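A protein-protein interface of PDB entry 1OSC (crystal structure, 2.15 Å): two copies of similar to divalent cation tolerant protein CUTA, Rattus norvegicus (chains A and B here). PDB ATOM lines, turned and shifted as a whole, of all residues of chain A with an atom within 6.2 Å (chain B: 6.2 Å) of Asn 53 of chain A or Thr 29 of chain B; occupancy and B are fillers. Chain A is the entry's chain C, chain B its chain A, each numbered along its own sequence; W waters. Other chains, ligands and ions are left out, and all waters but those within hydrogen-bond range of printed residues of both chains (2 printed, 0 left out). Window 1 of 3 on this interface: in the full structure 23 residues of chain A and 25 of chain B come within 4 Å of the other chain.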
ATOM      1  N   CYS A  51     -24.352  -2.328  10.715  1.00  0.00           N
ATOM      2  CA  CYS A  51     -23.843  -3.349   9.794  1.00  0.00           C
ATOM      3  C   CYS A  51     -23.109  -2.560   8.769  1.00  0.00           C
ATOM      4  O   CYS A  51     -23.562  -1.446   8.416  1.00  0.00           O
ATOM      5  CB  CYS A  51     -24.991  -4.152   9.123  1.00  0.00           C
ATOM      6  SG  CYS A  51     -24.203  -5.378   8.086  1.00  0.00           S
ATOM      7  N   VAL A  52     -21.987  -3.092   8.296  1.00  0.00           N
ATOM      8  CA  VAL A  52     -21.215  -2.481   7.244  1.00  0.00           C
ATOM      9  C   VAL A  52     -20.848  -3.522   6.172  1.00  0.00           C
ATOM     10  O   VAL A  52     -20.413  -4.634   6.534  1.00  0.00           O
ATOM     11  CB  VAL A  52     -19.873  -1.939   7.760  1.00  0.00           C
ATOM     12  CG1 VAL A  52     -19.145  -1.224   6.502  1.00  0.00           C
ATOM     13  CG2 VAL A  52     -20.090  -0.940   8.928  1.00  0.00           C
ATOM     14  N   ASN A  53     -21.098  -3.238   4.878  1.00  0.00           N
ATOM     15  CA  ASN A  53     -20.597  -4.116   3.824  1.00  0.00           C
ATOM     16  C   ASN A  53     -19.487  -3.491   3.088  1.00  0.00           C
ATOM     17  O   ASN A  53     -19.611  -2.353   2.749  1.00  0.00           O
ATOM     18  CB  ASN A  53     -21.670  -4.533   2.825  1.00  0.00           C
ATOM     19  CG  ASN A  53     -22.955  -5.073   3.508  1.00  0.00           C
ATOM     20  OD1 ASN A  53     -22.991  -6.182   3.954  1.00  0.00           O
ATOM     21  ND2 ASN A  53     -23.958  -4.243   3.602  1.00  0.00           N
ATOM     22  N   LEU A  54     -18.383  -4.201   2.850  1.00  0.00           N
ATOM     23  CA  LEU A  54     -17.276  -3.589   2.132  1.00  0.00           C
ATOM     24  C   LEU A  54     -17.243  -4.207   0.788  1.00  0.00           C
ATOM     25  O   LEU A  54     -17.339  -5.418   0.674  1.00  0.00           O
ATOM     26  CB  LEU A  54     -16.004  -3.894   2.843  1.00  0.00           C
ATOM     27  CG  LEU A  54     -15.888  -3.551   4.334  1.00  0.00           C
ATOM     28  CD1 LEU A  54     -14.458  -3.586   4.528  1.00  0.00           C
ATOM     29  CD2 LEU A  54     -16.322  -2.091   4.598  1.00  0.00           C
ATOM     30  N   ILE A  55     -17.243  -3.379  -0.221  1.00  0.00           N
ATOM     31  CA  ILE A  55     -17.209  -3.782  -1.573  1.00  0.00           C
ATOM     32  C   ILE A  55     -15.824  -3.447  -2.121  1.00  0.00           C
ATOM     33  O   ILE A  55     -15.494  -2.257  -2.368  1.00  0.00           O
ATOM     34  CB  ILE A  55     -18.308  -3.036  -2.405  1.00  0.00           C
ATOM     35  CG1 ILE A  55     -19.713  -3.329  -1.861  1.00  0.00           C
ATOM     36  CG2 ILE A  55     -18.152  -3.433  -3.816  1.00  0.00           C
ATOM     37  CD1 ILE A  55     -20.723  -2.110  -2.043  1.00  0.00           C
ATOM     38  N   LEU A  75     -15.518   0.514  -1.281  1.00  0.00           N
ATOM     39  CA  LEU A  75     -16.779   1.264  -1.050  1.00  0.00           C
ATOM     40  C   LEU A  75     -17.434   0.623   0.140  1.00  0.00           C
ATOM     41  O   LEU A  75     -17.568  -0.599   0.218  1.00  0.00           O
ATOM     42  CB  LEU A  75     -17.674   1.237  -2.350  1.00  0.00           C
ATOM     43  CG  LEU A  75     -19.148   1.795  -2.267  1.00  0.00           C
ATOM     44  CD1 LEU A  75     -19.119   3.309  -1.905  1.00  0.00           C
ATOM     45  CD2 LEU A  75     -19.871   1.572  -3.654  1.00  0.00           C
ATOM     46  N   MET A  76     -17.748   1.394   1.157  1.00  0.00           N
ATOM     47  CA  MET A  76     -18.401   0.840   2.268  1.00  0.00           C
ATOM     48  C   MET A  76     -19.866   1.238   2.188  1.00  0.00           C
ATOM     49  O   MET A  76     -20.216   2.390   1.838  1.00  0.00           O
ATOM     50  CB  MET A  76     -17.901   1.521   3.562  1.00  0.00           C
ATOM     51  CG  MET A  76     -16.403   1.342   3.921  1.00  0.00           C
ATOM     52  SD  MET A  76     -16.087   2.477   5.410  1.00  0.00           S
ATOM     53  CE  MET A  76     -16.804   1.552   6.613  1.00  0.00           C
ATOM     54  N   MET A  77     -20.708   0.341   2.605  1.00  0.00           N
ATOM     55  CA  MET A  77     -22.125   0.603   2.659  1.00  0.00           C
ATOM     56  C   MET A  77     -22.630   0.335   4.089  1.00  0.00           C
ATOM     57  O   MET A  77     -22.558  -0.760   4.552  1.00  0.00           O
ATOM     58  CB  MET A  77     -22.867  -0.331   1.720  1.00  0.00           C
ATOM     59  CG  MET A  77     -24.454  -0.041   1.805  1.00  0.00           C
ATOM     60  SD  MET A  77     -25.325  -1.060   0.539  1.00  0.00           S
ATOM     61  CE  MET A  77     -26.925  -0.626   0.888  1.00  0.00           C
ATOM     62  N   ILE A  78     -23.160   1.343   4.792  1.00  0.00           N
ATOM     63  CA  ILE A  78     -23.346   1.200   6.217  1.00  0.00           C
ATOM     64  C   ILE A  78     -24.820   1.379   6.559  1.00  0.00           C
ATOM     65  O   ILE A  78     -25.369   2.417   6.182  1.00  0.00           O
ATOM     66  CB  ILE A  78     -22.535   2.389   6.857  1.00  0.00           C
ATOM     67  CG1 ILE A  78     -21.017   2.380   6.436  1.00  0.00           C
ATOM     68  CG2 ILE A  78     -22.795   2.432   8.346  1.00  0.00           C
ATOM     69  CD1 ILE A  78     -20.243   3.649   7.050  1.00  0.00           C
ATOM     70  N   LYS A  79     -25.466   0.428   7.215  1.00  0.00           N
ATOM     71  CA  LYS A  79     -26.819   0.604   7.656  1.00  0.00           C
ATOM     72  C   LYS A  79     -26.859   1.114   9.070  1.00  0.00           C
ATOM     73  O   LYS A  79     -26.190   0.584   9.971  1.00  0.00           O
ATOM     74  CB  LYS A  79     -27.670  -0.657   7.488  1.00  0.00           C
ATOM     75  CG  LYS A  79     -28.012  -1.167   6.001  1.00  0.00           C
ATOM     76  CD  LYS A  79     -26.859  -1.218   4.991  1.00  0.00           C
ATOM     77  CE  LYS A  79     -25.934  -2.488   5.064  1.00  0.00           C
ATOM     78  NZ  LYS A  79     -26.590  -3.690   5.636  1.00  0.00           N
ATOM     79  N   PHE B  27     -31.808  -4.143  -1.580  1.00  0.00           N
ATOM     80  CA  PHE B  27     -30.492  -4.738  -1.372  1.00  0.00           C
ATOM     81  C   PHE B  27     -30.664  -5.867  -0.391  1.00  0.00           C
ATOM     82  O   PHE B  27     -31.202  -5.672   0.657  1.00  0.00           O
ATOM     83  CB  PHE B  27     -29.567  -3.791  -0.749  1.00  0.00           C
ATOM     84  CG  PHE B  27     -29.022  -2.750  -1.673  1.00  0.00           C
ATOM     85  CD1 PHE B  27     -29.644  -1.564  -1.791  1.00  0.00           C
ATOM     86  CD2 PHE B  27     -27.875  -2.966  -2.334  1.00  0.00           C
ATOM     87  CE1 PHE B  27     -29.142  -0.592  -2.676  1.00  0.00           C
ATOM     88  CE2 PHE B  27     -27.328  -1.996  -3.209  1.00  0.00           C
ATOM     89  CZ  PHE B  27     -27.986  -0.777  -3.330  1.00  0.00           C
ATOM     90  N   VAL B  28     -30.082  -7.003  -0.727  1.00  0.00           N
ATOM     91  CA  VAL B  28     -30.199  -8.232   0.063  1.00  0.00           C
ATOM     92  C   VAL B  28     -28.803  -8.894   0.205  1.00  0.00           C
ATOM     93  O   VAL B  28     -28.043  -9.044  -0.725  1.00  0.00           O
ATOM     94  CB  VAL B  28     -31.148  -9.194  -0.670  1.00  0.00           C
ATOM     95  CG1 VAL B  28     -31.302 -10.428  -0.005  1.00  0.00           C
ATOM     96  CG2 VAL B  28     -32.593  -8.626  -0.732  1.00  0.00           C
ATOM     97  N   THR B  29     -28.493  -9.275   1.381  1.00  0.00           N
ATOM     98  CA  THR B  29     -27.202  -9.892   1.654  1.00  0.00           C
ATOM     99  C   THR B  29     -27.345 -11.450   1.741  1.00  0.00           C
ATOM    100  O   THR B  29     -28.236 -11.933   2.439  1.00  0.00           O
ATOM    101  CB  THR B  29     -26.639  -9.241   2.926  1.00  0.00           C
ATOM    102  OG1 THR B  29     -25.798  -8.135   2.541  1.00  0.00           O
ATOM    103  CG2 THR B  29     -25.632 -10.099   3.486  1.00  0.00           C
ATOM    104  N   CYS B  30     -26.559 -12.196   0.952  1.00  0.00           N
ATOM    105  CA  CYS B  30     -26.582 -13.656   0.984  1.00  0.00           C
ATOM    106  C   CYS B  30     -25.256 -14.209   1.477  1.00  0.00           C
ATOM    107  O   CYS B  30     -24.170 -13.602   1.273  1.00  0.00           O
ATOM    108  CB  CYS B  30     -26.873 -14.245  -0.398  1.00  0.00           C
ATOM    109  SG  CYS B  30     -28.613 -14.034  -0.838  1.00  0.00           S
ATOM    110  N   PRO B  31     -25.322 -15.394   2.091  1.00  0.00           N
ATOM    111  CA  PRO B  31     -24.122 -16.012   2.655  1.00  0.00           C
ATOM    112  C   PRO B  31     -23.157 -16.461   1.546  1.00  0.00           C
ATOM    113  O   PRO B  31     -21.987 -16.428   1.820  1.00  0.00           O
ATOM    114  CB  PRO B  31     -24.700 -17.223   3.374  1.00  0.00           C
ATOM    115  CG  PRO B  31     -25.870 -17.619   2.464  1.00  0.00           C
ATOM    116  CD  PRO B  31     -26.502 -16.284   2.165  1.00  0.00           C
ATOM    117  N   ILE B  58     -17.970  -9.507  -1.083  1.00  0.00           N
ATOM    118  CA  ILE B  58     -18.181  -8.617   0.008  1.00  0.00           C
ATOM    119  C   ILE B  58     -17.845  -9.121   1.411  1.00  0.00           C
ATOM    120  O   ILE B  58     -17.944 -10.298   1.714  1.00  0.00           O
ATOM    121  CB  ILE B  58     -19.635  -7.842  -0.036  1.00  0.00           C
ATOM    122  CG1 ILE B  58     -20.636  -8.514   0.814  1.00  0.00           C
ATOM    123  CG2 ILE B  58     -20.062  -7.310  -1.547  1.00  0.00           C
ATOM    124  CD1 ILE B  58     -21.435  -7.653   1.545  1.00  0.00           C
ATOM    125  N   THR B  59     -17.436  -8.202   2.246  1.00  0.00           N
ATOM    126  CA  THR B  59     -17.183  -8.448   3.692  1.00  0.00           C
ATOM    127  C   THR B  59     -18.111  -7.681   4.587  1.00  0.00           C
ATOM    128  O   THR B  59     -18.195  -6.501   4.479  1.00  0.00           O
ATOM    129  CB  THR B  59     -15.740  -7.907   3.986  1.00  0.00           C
ATOM    130  OG1 THR B  59     -14.816  -8.762   3.297  1.00  0.00           O
ATOM    131  CG2 THR B  59     -15.394  -8.071   5.401  1.00  0.00           C
ATOM    132  N   SER B  60     -18.831  -8.342   5.472  1.00  0.00           N
ATOM    133  CA  SER B  60     -19.741  -7.736   6.400  1.00  0.00           C
ATOM    134  C   SER B  60     -19.286  -7.858   7.834  1.00  0.00           C
ATOM    135  O   SER B  60     -18.879  -8.933   8.254  1.00  0.00           O
ATOM    136  CB  SER B  60     -21.095  -8.465   6.334  1.00  0.00           C
ATOM    137  OG  SER B  60     -21.468  -8.406   4.990  1.00  0.00           O
ATOM    138  N   ILE B  61     -19.447  -6.764   8.537  1.00  0.00           N
ATOM    139  CA  ILE B  61     -18.977  -6.483   9.820  1.00  0.00           C
ATOM    140  C   ILE B  61     -20.131  -5.963  10.625  1.00  0.00           C
ATOM    141  O   ILE B  61     -20.801  -4.927  10.243  1.00  0.00           O
ATOM    142  CB  ILE B  61     -17.798  -5.426   9.773  1.00  0.00           C
ATOM    143  CG1 ILE B  61     -16.544  -6.065   9.160  1.00  0.00           C
ATOM    144  CG2 ILE B  61     -17.432  -5.136  11.199  1.00  0.00           C
ATOM    145  CD1 ILE B  61     -15.634  -5.192   8.302  1.00  0.00           C
ATOM    146  N   GLU B  73     -19.645 -12.514   2.219  1.00  0.00           N
ATOM    147  CA  GLU B  73     -20.964 -12.642   1.574  1.00  0.00           C
ATOM    148  C   GLU B  73     -21.048 -12.136   0.124  1.00  0.00           C
ATOM    149  O   GLU B  73     -20.039 -11.735  -0.461  1.00  0.00           O
ATOM    150  CB  GLU B  73     -21.949 -11.837   2.328  1.00  0.00           C
ATOM    151  CG  GLU B  73     -21.644 -11.644   3.781  1.00  0.00           C
ATOM    152  CD  GLU B  73     -22.863 -11.909   4.561  1.00  0.00           C
ATOM    153  OE1 GLU B  73     -23.240 -13.094   4.614  1.00  0.00           O
ATOM    154  OE2 GLU B  73     -23.475 -10.936   5.047  1.00  0.00           O
ATOM    155  N   VAL B  74     -22.288 -12.123  -0.382  1.00  0.00           N
ATOM    156  CA  VAL B  74     -22.665 -11.617  -1.704  1.00  0.00           C
ATOM    157  C   VAL B  74     -23.827 -10.563  -1.488  1.00  0.00           C
ATOM    158  O   VAL B  74     -24.727 -10.770  -0.637  1.00  0.00           O
ATOM    159  CB  VAL B  74     -23.084 -12.828  -2.598  1.00  0.00           C
ATOM    160  CG1 VAL B  74     -23.597 -12.400  -3.996  1.00  0.00           C
ATOM    161  CG2 VAL B  74     -21.845 -13.689  -2.894  1.00  0.00           C
ATOM    162  N   LEU B  75     -23.773  -9.417  -2.175  1.00  0.00           N
ATOM    163  CA  LEU B  75     -24.794  -8.407  -1.909  1.00  0.00           C
ATOM    164  C   LEU B  75     -25.616  -8.494  -3.243  1.00  0.00           C
ATOM    165  O   LEU B  75     -25.046  -8.542  -4.327  1.00  0.00           O
ATOM    166  CB  LEU B  75     -24.134  -7.038  -1.880  1.00  0.00           C
ATOM    167  CG  LEU B  75     -24.899  -5.723  -1.635  1.00  0.00           C
ATOM    168  CD1 LEU B  75     -25.829  -5.763  -0.383  1.00  0.00           C
ATOM    169  CD2 LEU B  75     -23.861  -4.507  -1.481  1.00  0.00           C
ATOM    170  N   MET B  76     -26.888  -8.536  -3.142  1.00  0.00           N
ATOM    171  CA  MET B  76     -27.758  -8.486  -4.328  1.00  0.00           C
ATOM    172  C   MET B  76     -28.424  -7.062  -4.404  1.00  0.00           C
ATOM    173  O   MET B  76     -28.965  -6.608  -3.445  1.00  0.00           O
ATOM    174  CB  MET B  76     -28.901  -9.487  -4.164  1.00  0.00           C
ATOM    175  CG  MET B  76     -28.454 -10.935  -3.828  1.00  0.00           C
ATOM    176  SD  MET B  76     -29.961 -12.040  -3.569  1.00  0.00           S
ATOM    177  CE  MET B  76     -30.125 -12.489  -5.195  1.00  0.00           C
ATOM    178  N   ALA B 101     -33.019 -12.387   7.603  1.00  0.00           N
ATOM    179  CA  ALA B 101     -32.834 -11.800   6.215  1.00  0.00           C
ATOM    180  C   ALA B 101     -32.760 -10.243   6.176  1.00  0.00           C
ATOM    181  O   ALA B 101     -33.573  -9.587   6.695  1.00  0.00           O
ATOM    182  CB  ALA B 101     -33.963 -12.281   5.255  1.00  0.00           C
ATOM    183  N   GLU B 102     -31.688  -9.737   5.674  1.00  0.00           N
ATOM    184  CA  GLU B 102     -31.427  -8.350   5.595  1.00  0.00           C
ATOM    185  C   GLU B 102     -31.956  -7.906   4.198  1.00  0.00           C
ATOM    186  O   GLU B 102     -31.377  -8.267   3.195  1.00  0.00           O
ATOM    187  CB  GLU B 102     -29.879  -8.194   5.752  1.00  0.00           C
ATOM    188  CG  GLU B 102     -29.464  -8.603   7.196  1.00  0.00           C
ATOM    189  CD  GLU B 102     -28.276  -9.609   7.407  1.00  0.00           C
ATOM    190  OE1 GLU B 102     -28.368 -10.361   8.440  1.00  0.00           O
ATOM    191  OE2 GLU B 102     -27.258  -9.642   6.605  1.00  0.00           O
ATOM    192  N   VAL B 103     -33.105  -7.237   4.195  1.00  0.00           N
ATOM    193  CA  VAL B 103     -33.629  -6.574   3.001  1.00  0.00           C
ATOM    194  C   VAL B 103     -33.978  -5.153   3.357  1.00  0.00           C
ATOM    195  O   VAL B 103     -34.511  -4.935   4.396  1.00  0.00           O
ATOM    196  CB  VAL B 103     -34.734  -7.414   2.203  1.00  0.00           C
ATOM    197  CG1 VAL B 103     -35.118  -8.633   2.909  1.00  0.00           C
ATOM    198  CG2 VAL B 103     -35.826  -6.679   1.627  1.00  0.00           C
HETATM  199  O   HOH W   1     -25.719  -7.081   6.035  1.00  0.00           O
HETATM  200  O   HOH W   2     -25.931  -8.256   9.444  1.00  0.00           O
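Asn 53 of chain A touches just these residues of chain B: Thr 29 (3.7 Å), Ile 58 (3.2 Å), Thr 59 (3.4 Å) and Ser 60 (2.9 Å). Printed residues of chain B within 4 Å of Leu 54 of chain A: Ile 58 (3.4 Å) and Thr 59 (2.8 Å). Of the printed residues of chain B, Ile 55 of chain A touches Leu 75. Printed residues of chain B within 4 Å of Met 77 of chain A: Phe 27 (3.9 Å). Printed residues of chain A within 4 Å of Thr 29 of chain B: Asn 53 (3.7 Å). The nearest residue of chain B that does not touch Asn 53 of chain A is Leu 75 of chain B (4.7 Å). The nearest printed residue of chain B that does not touch Met 77 of chain A is Leu 75 of chain B (4.3 Å).
Of the 10 printed residues of chain A, 6 touch a printed residue of chain B. Printed residues of chain A that touch a printed residue of chain B: Cys 51, Val 52, Asn 53, Leu 54, Ile 55 and Met 77. Hydrophobic or aromatic side chains of chain A that line the printed part of chain B: Val 52, Leu 54, Ile 55 and Met 77. Of the 16 printed residues of chain B, 7 touch a printed residue of chain A. Printed residues of chain B that touch a printed residue of chain A: Phe 27, Thr 29, Ile 58, Thr 59, Ser 60, Ile 61 and Leu 75. Hydrophobic or aromatic side chains of chain B within 4 Å of the printed part of chain A: Phe 27, Ile 58 and Leu 75. Among the printed residues, no Asp or Glu carboxylate lies within 4 Å of a Lys or Arg side-chain nitrogen of the other chain.
Water W1 lies within hydrogen-bond range of OE2 of Glu 102 of chain B (3.0 Å) and SG of Cys 51 of chain A (3.1 Å). Water W2 lies within hydrogen-bond range of the side-chain carboxylate (OE1) of Glu 102 of chain B (3.4 Å) and the side-chain sulfur (SG) of Cys 51 of chain A (3.6 Å).
The side-chain hydroxyl of Ser 60 of chain B is in hydrogen-bond range of the side-chain amide oxygen of Asn 53 of chain A, at 2.9 Å. O of Thr 59 of chain B is in hydrogen-bond range of N of Leu 54 of chain A (2.8 Å). O of Ile 61 of chain B is in hydrogen-bond range of N of Val 52 of chain A (2.9 Å).
O of Ile 61 of chain B touches CA of Cys 51 of chain A (3.5 Å). Val 52 of chain A touches Thr 59 of chain B. Val 52 of chain A touches Ser 60 of chain B. Asn 53 of chain A touches Thr 29 of chain B. Asn 53 of chain A touches Ile 58 of chain B (OD1 to CD1, 3.2 Å). Thr 59 of chain B touches Asn 53 of chain A. Leu 54 of chain A touches Ile 58 of chain B. CD2 of Leu 75 of chain B touches CD1 of Ile 55 of chain A, at 3.99 Å. Met 77 of chain A touches Phe 27 of chain B (CE to CD1, 3.9 Å).
ND2 of Asn 53 of chain A sits close to NZ of Lys 79 of chain A (3.4 Å). The side-chain hydroxyl of Ser 60 of chain B lies within hydrogen-bond range of the side-chain carboxylate of Glu 73 of chain B (3.2 Å). O of Cys 51 of chain A lies within hydrogen-bond range of N of Lys 79 of chain A. O of Ile 58 of chain B sits at hydrogen-bond distance from N of Glu 73 of chain B. O of Leu 75 of chain A is in hydrogen-bond range of N of Ile 55 of chain A. O of Met 77 of chain A sits at hydrogen-bond distance from N of Asn 53 of chain A (2.9 Å).
2 positions are printed for both chains. Of the 12 pairs that touch across the chains among the printed residues, none has its exchanged pair printed and touching as well.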
